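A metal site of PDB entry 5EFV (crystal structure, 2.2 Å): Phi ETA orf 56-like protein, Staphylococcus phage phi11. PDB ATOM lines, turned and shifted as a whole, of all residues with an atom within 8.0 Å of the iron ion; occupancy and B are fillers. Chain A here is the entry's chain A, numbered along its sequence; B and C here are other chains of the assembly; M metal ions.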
ATOM      1  N   LEU A  51      -7.135  10.305  -1.999  1.00  0.00           N
ATOM      2  CA  LEU A  51      -8.014  11.164  -2.788  1.00  0.00           C
ATOM      3  C   LEU A  51      -7.297  11.638  -4.044  1.00  0.00           C
ATOM      4  O   LEU A  51      -7.887  11.615  -5.141  1.00  0.00           O
ATOM      5  CB  LEU A  51      -8.495  12.392  -1.987  1.00  0.00           C
ATOM      6  CG  LEU A  51      -9.765  12.312  -1.167  1.00  0.00           C
ATOM      7  CD1 LEU A  51      -9.706  13.369  -0.041  1.00  0.00           C
ATOM      8  CD2 LEU A  51     -11.016  12.492  -2.026  1.00  0.00           C
ATOM      9  N   HIS A  54      -6.893   8.693  -6.373  1.00  0.00           N
ATOM     10  CA  HIS A  54      -8.182   8.360  -6.945  1.00  0.00           C
ATOM     11  C   HIS A  54      -8.473   9.230  -8.177  1.00  0.00           C
ATOM     12  O   HIS A  54      -8.842   8.736  -9.242  1.00  0.00           O
ATOM     13  CB  HIS A  54      -9.301   8.512  -5.891  1.00  0.00           C
ATOM     14  CG  HIS A  54     -10.666   8.206  -6.439  1.00  0.00           C
ATOM     15  ND1 HIS A  54     -11.005   6.925  -6.894  1.00  0.00           N
ATOM     16  CD2 HIS A  54     -11.739   9.012  -6.578  1.00  0.00           C
ATOM     17  CE1 HIS A  54     -12.263   6.996  -7.304  1.00  0.00           C
ATOM     18  NE2 HIS A  54     -12.753   8.216  -7.141  1.00  0.00           N
ATOM     19  N   ARG A  55      -8.277  10.537  -8.016  1.00  0.00           N
ATOM     20  CA  ARG A  55      -8.489  11.530  -9.036  1.00  0.00           C
ATOM     21  C   ARG A  55      -7.577  11.399 -10.270  1.00  0.00           C
ATOM     22  O   ARG A  55      -8.042  11.507 -11.404  1.00  0.00           O
ATOM     23  CB  ARG A  55      -8.282  12.931  -8.453  1.00  0.00           C
ATOM     24  CG  ARG A  55      -9.383  13.419  -7.549  1.00  0.00           C
ATOM     25  CD  ARG A  55      -9.064  14.780  -6.955  1.00  0.00           C
ATOM     26  NE  ARG A  55     -10.297  15.386  -6.398  1.00  0.00           N
ATOM     27  CZ  ARG A  55     -10.509  15.659  -5.125  1.00  0.00           C
ATOM     28  NH1 ARG A  55      -9.566  15.452  -4.219  1.00  0.00           N
ATOM     29  NH2 ARG A  55     -11.664  16.189  -4.742  1.00  0.00           N
ATOM     30  N   GLU A  58      -5.257   6.290 -10.079  1.00  0.00           N
ATOM     31  CA  GLU A  58      -5.902   5.011  -9.860  1.00  0.00           C
ATOM     32  C   GLU A  58      -6.447   4.426 -11.158  1.00  0.00           C
ATOM     33  O   GLU A  58      -7.198   5.111 -11.871  1.00  0.00           O
ATOM     34  CB  GLU A  58      -7.018   5.174  -8.826  1.00  0.00           C
ATOM     35  CG  GLU A  58      -7.727   3.883  -8.483  1.00  0.00           C
ATOM     36  CD  GLU A  58      -8.683   4.040  -7.325  1.00  0.00           C
ATOM     37  OE1 GLU A  58      -9.137   3.007  -6.804  1.00  0.00           O
ATOM     38  OE2 GLU A  58      -8.989   5.198  -6.950  1.00  0.00           O
ATOM     39  N   ALA A  61     -10.567   3.519 -11.146  1.00  0.00           N
ATOM     40  CA  ALA A  61     -11.078   4.393 -10.103  1.00  0.00           C
ATOM     41  C   ALA A  61     -12.549   4.028  -9.946  1.00  0.00           C
ATOM     42  O   ALA A  61     -13.087   4.089  -8.840  1.00  0.00           O
ATOM     43  CB  ALA A  61     -10.978   5.836 -10.557  1.00  0.00           C
ATOM     44  N   HIS A  62     -13.208   3.640 -11.088  1.00  0.00           N
ATOM     45  CA  HIS A  62     -14.622   3.245 -11.139  1.00  0.00           C
ATOM     46  C   HIS A  62     -14.877   2.249 -12.263  1.00  0.00           C
ATOM     47  O   HIS A  62     -14.054   2.122 -13.164  1.00  0.00           O
ATOM     48  CB  HIS A  62     -15.523   4.479 -11.367  1.00  0.00           C
ATOM     49  CG  HIS A  62     -15.489   5.463 -10.231  1.00  0.00           C
ATOM     50  ND1 HIS A  62     -16.111   5.191  -9.012  1.00  0.00           N
ATOM     51  CD2 HIS A  62     -14.888   6.675 -10.161  1.00  0.00           C
ATOM     52  CE1 HIS A  62     -15.868   6.248  -8.255  1.00  0.00           C
ATOM     53  NE2 HIS A  62     -15.143   7.163  -8.888  1.00  0.00           N
ATOM     54  N   GLN A  66     -21.039   2.747 -12.934  1.00  0.00           N
ATOM     55  CA  GLN A  66     -21.164   3.760 -11.883  1.00  0.00           C
ATOM     56  C   GLN A  66     -21.282   5.174 -12.471  1.00  0.00           C
ATOM     57  O   GLN A  66     -21.504   6.108 -11.721  1.00  0.00           O
ATOM     58  CB  GLN A  66     -19.936   3.713 -10.969  1.00  0.00           C
ATOM     59  CG  GLN A  66     -19.740   2.367 -10.253  1.00  0.00           C
ATOM     60  CD  GLN A  66     -18.571   2.491  -9.322  1.00  0.00           C
ATOM     61  OE1 GLN A  66     -17.424   2.291  -9.724  1.00  0.00           O
ATOM     62  NE2 GLN A  66     -18.824   2.898  -8.090  1.00  0.00           N
ATOM     63  N   ILE A  67     -21.127   5.310 -13.790  1.00  0.00           N
ATOM     64  CA  ILE A  67     -21.136   6.596 -14.472  1.00  0.00           C
ATOM     65  C   ILE A  67     -22.425   6.847 -15.212  1.00  0.00           C
ATOM     66  O   ILE A  67     -22.815   6.099 -16.127  1.00  0.00           O
ATOM     67  CB  ILE A  67     -19.888   6.777 -15.394  1.00  0.00           C
ATOM     68  CG1 ILE A  67     -18.573   6.278 -14.714  1.00  0.00           C
ATOM     69  CG2 ILE A  67     -19.779   8.229 -15.920  1.00  0.00           C
ATOM     70  CD1 ILE A  67     -18.122   6.997 -13.279  1.00  0.00           C
ATOM     71  N   LEU B  51     -14.434  15.080  -0.964  1.00  0.00           N
ATOM     72  CA  LEU B  51     -15.100  13.900  -1.501  1.00  0.00           C
ATOM     73  C   LEU B  51     -16.493  14.252  -2.046  1.00  0.00           C
ATOM     74  O   LEU B  51     -16.835  13.774  -3.122  1.00  0.00           O
ATOM     75  CB  LEU B  51     -15.162  12.761  -0.475  1.00  0.00           C
ATOM     76  CG  LEU B  51     -15.802  11.416  -0.899  1.00  0.00           C
ATOM     77  CD1 LEU B  51     -15.187  10.859  -2.146  1.00  0.00           C
ATOM     78  CD2 LEU B  51     -15.674  10.392   0.203  1.00  0.00           C
ATOM     79  N   HIS B  54     -15.957  16.224  -5.230  1.00  0.00           N
ATOM     80  CA  HIS B  54     -15.475  15.281  -6.251  1.00  0.00           C
ATOM     81  C   HIS B  54     -16.663  14.556  -6.886  1.00  0.00           C
ATOM     82  O   HIS B  54     -16.743  14.474  -8.107  1.00  0.00           O
ATOM     83  CB  HIS B  54     -14.499  14.275  -5.617  1.00  0.00           C
ATOM     84  CG  HIS B  54     -14.090  13.147  -6.518  1.00  0.00           C
ATOM     85  ND1 HIS B  54     -13.339  13.369  -7.634  1.00  0.00           N
ATOM     86  CD2 HIS B  54     -14.328  11.826  -6.400  1.00  0.00           C
ATOM     87  CE1 HIS B  54     -13.141  12.185  -8.164  1.00  0.00           C
ATOM     88  NE2 HIS B  54     -13.744  11.233  -7.468  1.00  0.00           N
ATOM     89  N   ARG B  55     -17.595  14.077  -6.056  1.00  0.00           N
ATOM     90  CA  ARG B  55     -18.795  13.343  -6.482  1.00  0.00           C
ATOM     91  C   ARG B  55     -19.753  14.179  -7.320  1.00  0.00           C
ATOM     92  O   ARG B  55     -20.218  13.723  -8.358  1.00  0.00           O
ATOM     93  CB  ARG B  55     -19.559  12.832  -5.257  1.00  0.00           C
ATOM     94  CG  ARG B  55     -18.973  11.645  -4.546  1.00  0.00           C
ATOM     95  CD  ARG B  55     -19.890  11.260  -3.388  1.00  0.00           C
ATOM     96  NE  ARG B  55     -19.492   9.994  -2.773  1.00  0.00           N
ATOM     97  CZ  ARG B  55     -19.626   9.690  -1.488  1.00  0.00           C
ATOM     98  NH1 ARG B  55     -19.186   8.523  -1.022  1.00  0.00           N
ATOM     99  NH2 ARG B  55     -20.188  10.549  -0.647  1.00  0.00           N
ATOM    100  N   GLU B  58     -16.987  18.446  -9.251  1.00  0.00           N
ATOM    101  CA  GLU B  58     -15.692  18.451  -9.911  1.00  0.00           C
ATOM    102  C   GLU B  58     -15.766  18.144 -11.418  1.00  0.00           C
ATOM    103  O   GLU B  58     -16.282  17.093 -11.820  1.00  0.00           O
ATOM    104  CB  GLU B  58     -14.702  17.532  -9.191  1.00  0.00           C
ATOM    105  CG  GLU B  58     -13.298  17.631  -9.713  1.00  0.00           C
ATOM    106  CD  GLU B  58     -12.248  17.015  -8.806  1.00  0.00           C
ATOM    107  OE1 GLU B  58     -12.522  15.949  -8.216  1.00  0.00           O
ATOM    108  OE2 GLU B  58     -11.118  17.549  -8.753  1.00  0.00           O
ATOM    109  N   ALA B  61     -13.346  14.967 -12.807  1.00  0.00           N
ATOM    110  CA  ALA B  61     -13.254  14.190 -11.585  1.00  0.00           C
ATOM    111  C   ALA B  61     -12.293  13.045 -11.915  1.00  0.00           C
ATOM    112  O   ALA B  61     -11.549  12.615 -11.041  1.00  0.00           O
ATOM    113  CB  ALA B  61     -14.612  13.634 -11.206  1.00  0.00           C
ATOM    114  N   HIS B  62     -12.326  12.578 -13.184  1.00  0.00           N
ATOM    115  CA  HIS B  62     -11.513  11.458 -13.689  1.00  0.00           C
ATOM    116  C   HIS B  62     -11.239  11.584 -15.183  1.00  0.00           C
ATOM    117  O   HIS B  62     -11.900  12.348 -15.864  1.00  0.00           O
ATOM    118  CB  HIS B  62     -12.222  10.104 -13.436  1.00  0.00           C
ATOM    119  CG  HIS B  62     -12.403   9.762 -11.987  1.00  0.00           C
ATOM    120  ND1 HIS B  62     -11.325   9.361 -11.205  1.00  0.00           N
ATOM    121  CD2 HIS B  62     -13.513   9.792 -11.216  1.00  0.00           C
ATOM    122  CE1 HIS B  62     -11.814   9.165  -9.992  1.00  0.00           C
ATOM    123  NE2 HIS B  62     -13.129   9.394  -9.943  1.00  0.00           N
ATOM    124  N   GLN B  66      -9.324   5.756 -16.529  1.00  0.00           N
ATOM    125  CA  GLN B  66      -9.477   5.285 -15.141  1.00  0.00           C
ATOM    126  C   GLN B  66     -10.786   4.527 -14.959  1.00  0.00           C
ATOM    127  O   GLN B  66     -11.044   4.014 -13.872  1.00  0.00           O
ATOM    128  CB  GLN B  66      -9.528   6.507 -14.194  1.00  0.00           C
ATOM    129  CG  GLN B  66      -8.264   7.335 -14.179  1.00  0.00           C
ATOM    130  CD  GLN B  66      -8.391   8.397 -13.131  1.00  0.00           C
ATOM    131  OE1 GLN B  66      -8.929   9.484 -13.398  1.00  0.00           O
ATOM    132  NE2 GLN B  66      -7.924   8.121 -11.934  1.00  0.00           N
ATOM    133  N   ILE B  67     -11.656   4.543 -15.965  1.00  0.00           N
ATOM    134  CA  ILE B  67     -13.005   3.950 -15.892  1.00  0.00           C
ATOM    135  C   ILE B  67     -13.047   2.679 -16.689  1.00  0.00           C
ATOM    136  O   ILE B  67     -12.802   2.690 -17.893  1.00  0.00           O
ATOM    137  CB  ILE B  67     -14.111   4.975 -16.327  1.00  0.00           C
ATOM    138  CG1 ILE B  67     -13.878   6.393 -15.756  1.00  0.00           C
ATOM    139  CG2 ILE B  67     -15.515   4.443 -16.000  1.00  0.00           C
ATOM    140  CD1 ILE B  67     -14.047   6.619 -14.181  1.00  0.00           C
ATOM    141  N   LEU C  51     -15.142   6.795   1.098  1.00  0.00           N
ATOM    142  CA  LEU C  51     -14.254   6.737  -0.060  1.00  0.00           C
ATOM    143  C   LEU C  51     -14.299   5.358  -0.738  1.00  0.00           C
ATOM    144  O   LEU C  51     -14.357   5.306  -1.953  1.00  0.00           O
ATOM    145  CB  LEU C  51     -12.808   7.111   0.310  1.00  0.00           C
ATOM    146  CG  LEU C  51     -11.767   7.207  -0.851  1.00  0.00           C
ATOM    147  CD1 LEU C  51     -12.246   8.092  -2.044  1.00  0.00           C
ATOM    148  CD2 LEU C  51     -10.417   7.663  -0.316  1.00  0.00           C
ATOM    149  N   HIS C  54     -17.664   5.014  -2.459  1.00  0.00           N
ATOM    150  CA  HIS C  54     -17.611   5.831  -3.669  1.00  0.00           C
ATOM    151  C   HIS C  54     -16.919   5.050  -4.809  1.00  0.00           C
ATOM    152  O   HIS C  54     -17.445   4.960  -5.918  1.00  0.00           O
ATOM    153  CB  HIS C  54     -16.895   7.182  -3.417  1.00  0.00           C
ATOM    154  CG  HIS C  54     -16.699   7.998  -4.665  1.00  0.00           C
ATOM    155  ND1 HIS C  54     -17.770   8.517  -5.391  1.00  0.00           N
ATOM    156  CD2 HIS C  54     -15.547   8.363  -5.299  1.00  0.00           C
ATOM    157  CE1 HIS C  54     -17.255   9.155  -6.426  1.00  0.00           C
ATOM    158  NE2 HIS C  54     -15.922   9.093  -6.425  1.00  0.00           N
ATOM    159  N   ARG C  55     -15.750   4.463  -4.502  1.00  0.00           N
ATOM    160  CA  ARG C  55     -14.946   3.701  -5.458  1.00  0.00           C
ATOM    161  C   ARG C  55     -15.610   2.439  -5.996  1.00  0.00           C
ATOM    162  O   ARG C  55     -15.552   2.175  -7.206  1.00  0.00           O
ATOM    163  CB  ARG C  55     -13.647   3.259  -4.773  1.00  0.00           C
ATOM    164  CG  ARG C  55     -12.600   4.330  -4.646  1.00  0.00           C
ATOM    165  CD  ARG C  55     -11.381   3.684  -4.038  1.00  0.00           C
ATOM    166  NE  ARG C  55     -10.188   4.464  -4.301  1.00  0.00           N
ATOM    167  CZ  ARG C  55      -9.280   4.760  -3.387  1.00  0.00           C
ATOM    168  NH1 ARG C  55      -9.432   4.338  -2.138  1.00  0.00           N
ATOM    169  NH2 ARG C  55      -8.214   5.466  -3.722  1.00  0.00           N
ATOM    170  N   GLU C  58     -21.011   2.941  -5.082  1.00  0.00           N
ATOM    171  CA  GLU C  58     -21.888   4.038  -5.435  1.00  0.00           C
ATOM    172  C   GLU C  58     -22.395   3.977  -6.902  1.00  0.00           C
ATOM    173  O   GLU C  58     -21.596   3.904  -7.849  1.00  0.00           O
ATOM    174  CB  GLU C  58     -21.241   5.385  -5.129  1.00  0.00           C
ATOM    175  CG  GLU C  58     -22.187   6.561  -5.256  1.00  0.00           C
ATOM    176  CD  GLU C  58     -21.625   7.909  -4.864  1.00  0.00           C
ATOM    177  OE1 GLU C  58     -20.415   8.006  -4.568  1.00  0.00           O
ATOM    178  OE2 GLU C  58     -22.403   8.893  -4.892  1.00  0.00           O
ATOM    179  N   ALA C  61     -21.669   7.421  -9.118  1.00  0.00           N
ATOM    180  CA  ALA C  61     -20.511   7.949  -8.405  1.00  0.00           C
ATOM    181  C   ALA C  61     -20.196   9.254  -9.083  1.00  0.00           C
ATOM    182  O   ALA C  61     -19.726  10.166  -8.446  1.00  0.00           O
ATOM    183  CB  ALA C  61     -19.342   6.992  -8.551  1.00  0.00           C
ATOM    184  N   HIS C  62     -20.476   9.345 -10.426  1.00  0.00           N
ATOM    185  CA  HIS C  62     -20.230  10.523 -11.271  1.00  0.00           C
ATOM    186  C   HIS C  62     -21.189  10.607 -12.436  1.00  0.00           C
ATOM    187  O   HIS C  62     -21.827   9.627 -12.785  1.00  0.00           O
ATOM    188  CB  HIS C  62     -18.781  10.486 -11.845  1.00  0.00           C
ATOM    189  CG  HIS C  62     -17.706  10.571 -10.800  1.00  0.00           C
ATOM    190  ND1 HIS C  62     -17.410  11.766 -10.161  1.00  0.00           N
ATOM    191  CD2 HIS C  62     -16.899   9.599 -10.296  1.00  0.00           C
ATOM    192  CE1 HIS C  62     -16.450  11.488  -9.296  1.00  0.00           C
ATOM    193  NE2 HIS C  62     -16.082  10.203  -9.356  1.00  0.00           N
ATOM    194  N   GLN C  66     -18.304  14.792 -16.112  1.00  0.00           N
ATOM    195  CA  GLN C  66     -17.165  14.939 -15.177  1.00  0.00           C
ATOM    196  C   GLN C  66     -15.990  14.083 -15.624  1.00  0.00           C
ATOM    197  O   GLN C  66     -14.931  14.136 -14.986  1.00  0.00           O
ATOM    198  CB  GLN C  66     -17.562  14.441 -13.790  1.00  0.00           C
ATOM    199  CG  GLN C  66     -18.689  15.225 -13.135  1.00  0.00           C
ATOM    200  CD  GLN C  66     -18.896  14.694 -11.739  1.00  0.00           C
ATOM    201  OE1 GLN C  66     -19.606  13.718 -11.546  1.00  0.00           O
ATOM    202  NE2 GLN C  66     -18.238  15.290 -10.763  1.00  0.00           N
ATOM    203  N   ILE C  67     -16.195  13.222 -16.648  1.00  0.00           N
ATOM    204  CA  ILE C  67     -15.179  12.293 -17.108  1.00  0.00           C
ATOM    205  C   ILE C  67     -14.600  12.791 -18.405  1.00  0.00           C
ATOM    206  O   ILE C  67     -15.306  12.950 -19.398  1.00  0.00           O
ATOM    207  CB  ILE C  67     -15.717  10.828 -17.197  1.00  0.00           C
ATOM    208  CG1 ILE C  67     -16.592  10.432 -15.970  1.00  0.00           C
ATOM    209  CG2 ILE C  67     -14.581   9.814 -17.456  1.00  0.00           C
ATOM    210  CD1 ILE C  67     -15.871  10.237 -14.554  1.00  0.00           C
HETATM  211 FE    FE M   1     -14.484   9.193  -8.241  1.00  0.00          FE
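The side-chain amide oxygen (OE1) of Gln 66 of chain C lies within hydrogen-bond range of a ring nitrogen (ND1) of His 62 of chain C (3.2 Å). NE of Arg 55 of chain B lies close to ND1 of His 54 of chain C, 3.5 Å away. ND1 of His 54 of chain B is in hydrogen-bond range of OE1 of Glu 58 of chain B (2.8 Å). OE1 of Glu 58 of chain C sits at hydrogen-bond distance from ND1 of His 54 of chain C (2.8 Å). The backbone carbonyl oxygen (O) of His 54 of chain B sits at hydrogen-bond distance from the side-chain amide nitrogen (NE2) of Gln 66 of chain C, 3.2 Å away. O of His 54 of chain C is in hydrogen-bond range of NE2 of Gln 66 of chain A (3.3 Å). ND1 of His 54 of chain A lies within hydrogen-bond range of OE2 of Glu 58 of chain A, at 2.7 Å. A ring nitrogen (ND1) of His 62 of chain B is in hydrogen-bond range of the side-chain amide oxygen (OE1) of Gln 66 of chain B (3.3 Å).
Six residues have an atom within 4 Å of the iron ion: His 54 of chain A, His 62 of chain A, His 54 of chain B, His 62 of chain B, His 54 of chain C and His 62 of chain C. The nearest printed residue that does not touch the iron ion is Ala 61 of chain B (5.3 Å).
NE2 of His 62 of chain B binds the iron ion. NE2 of His 62 of chain C is bound to the iron ion (2.2 Å). NE2 of His 62 of chain A is bound to the iron ion. NE2 of His 54 of chain A binds the iron ion (2.3 Å). The iron ion is bound by NE2 of His 54 of chain B, 2.3 Å away. NE2 of His 54 of chain C binds the iron ion. The iron ion has six donor atoms within binding distance.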
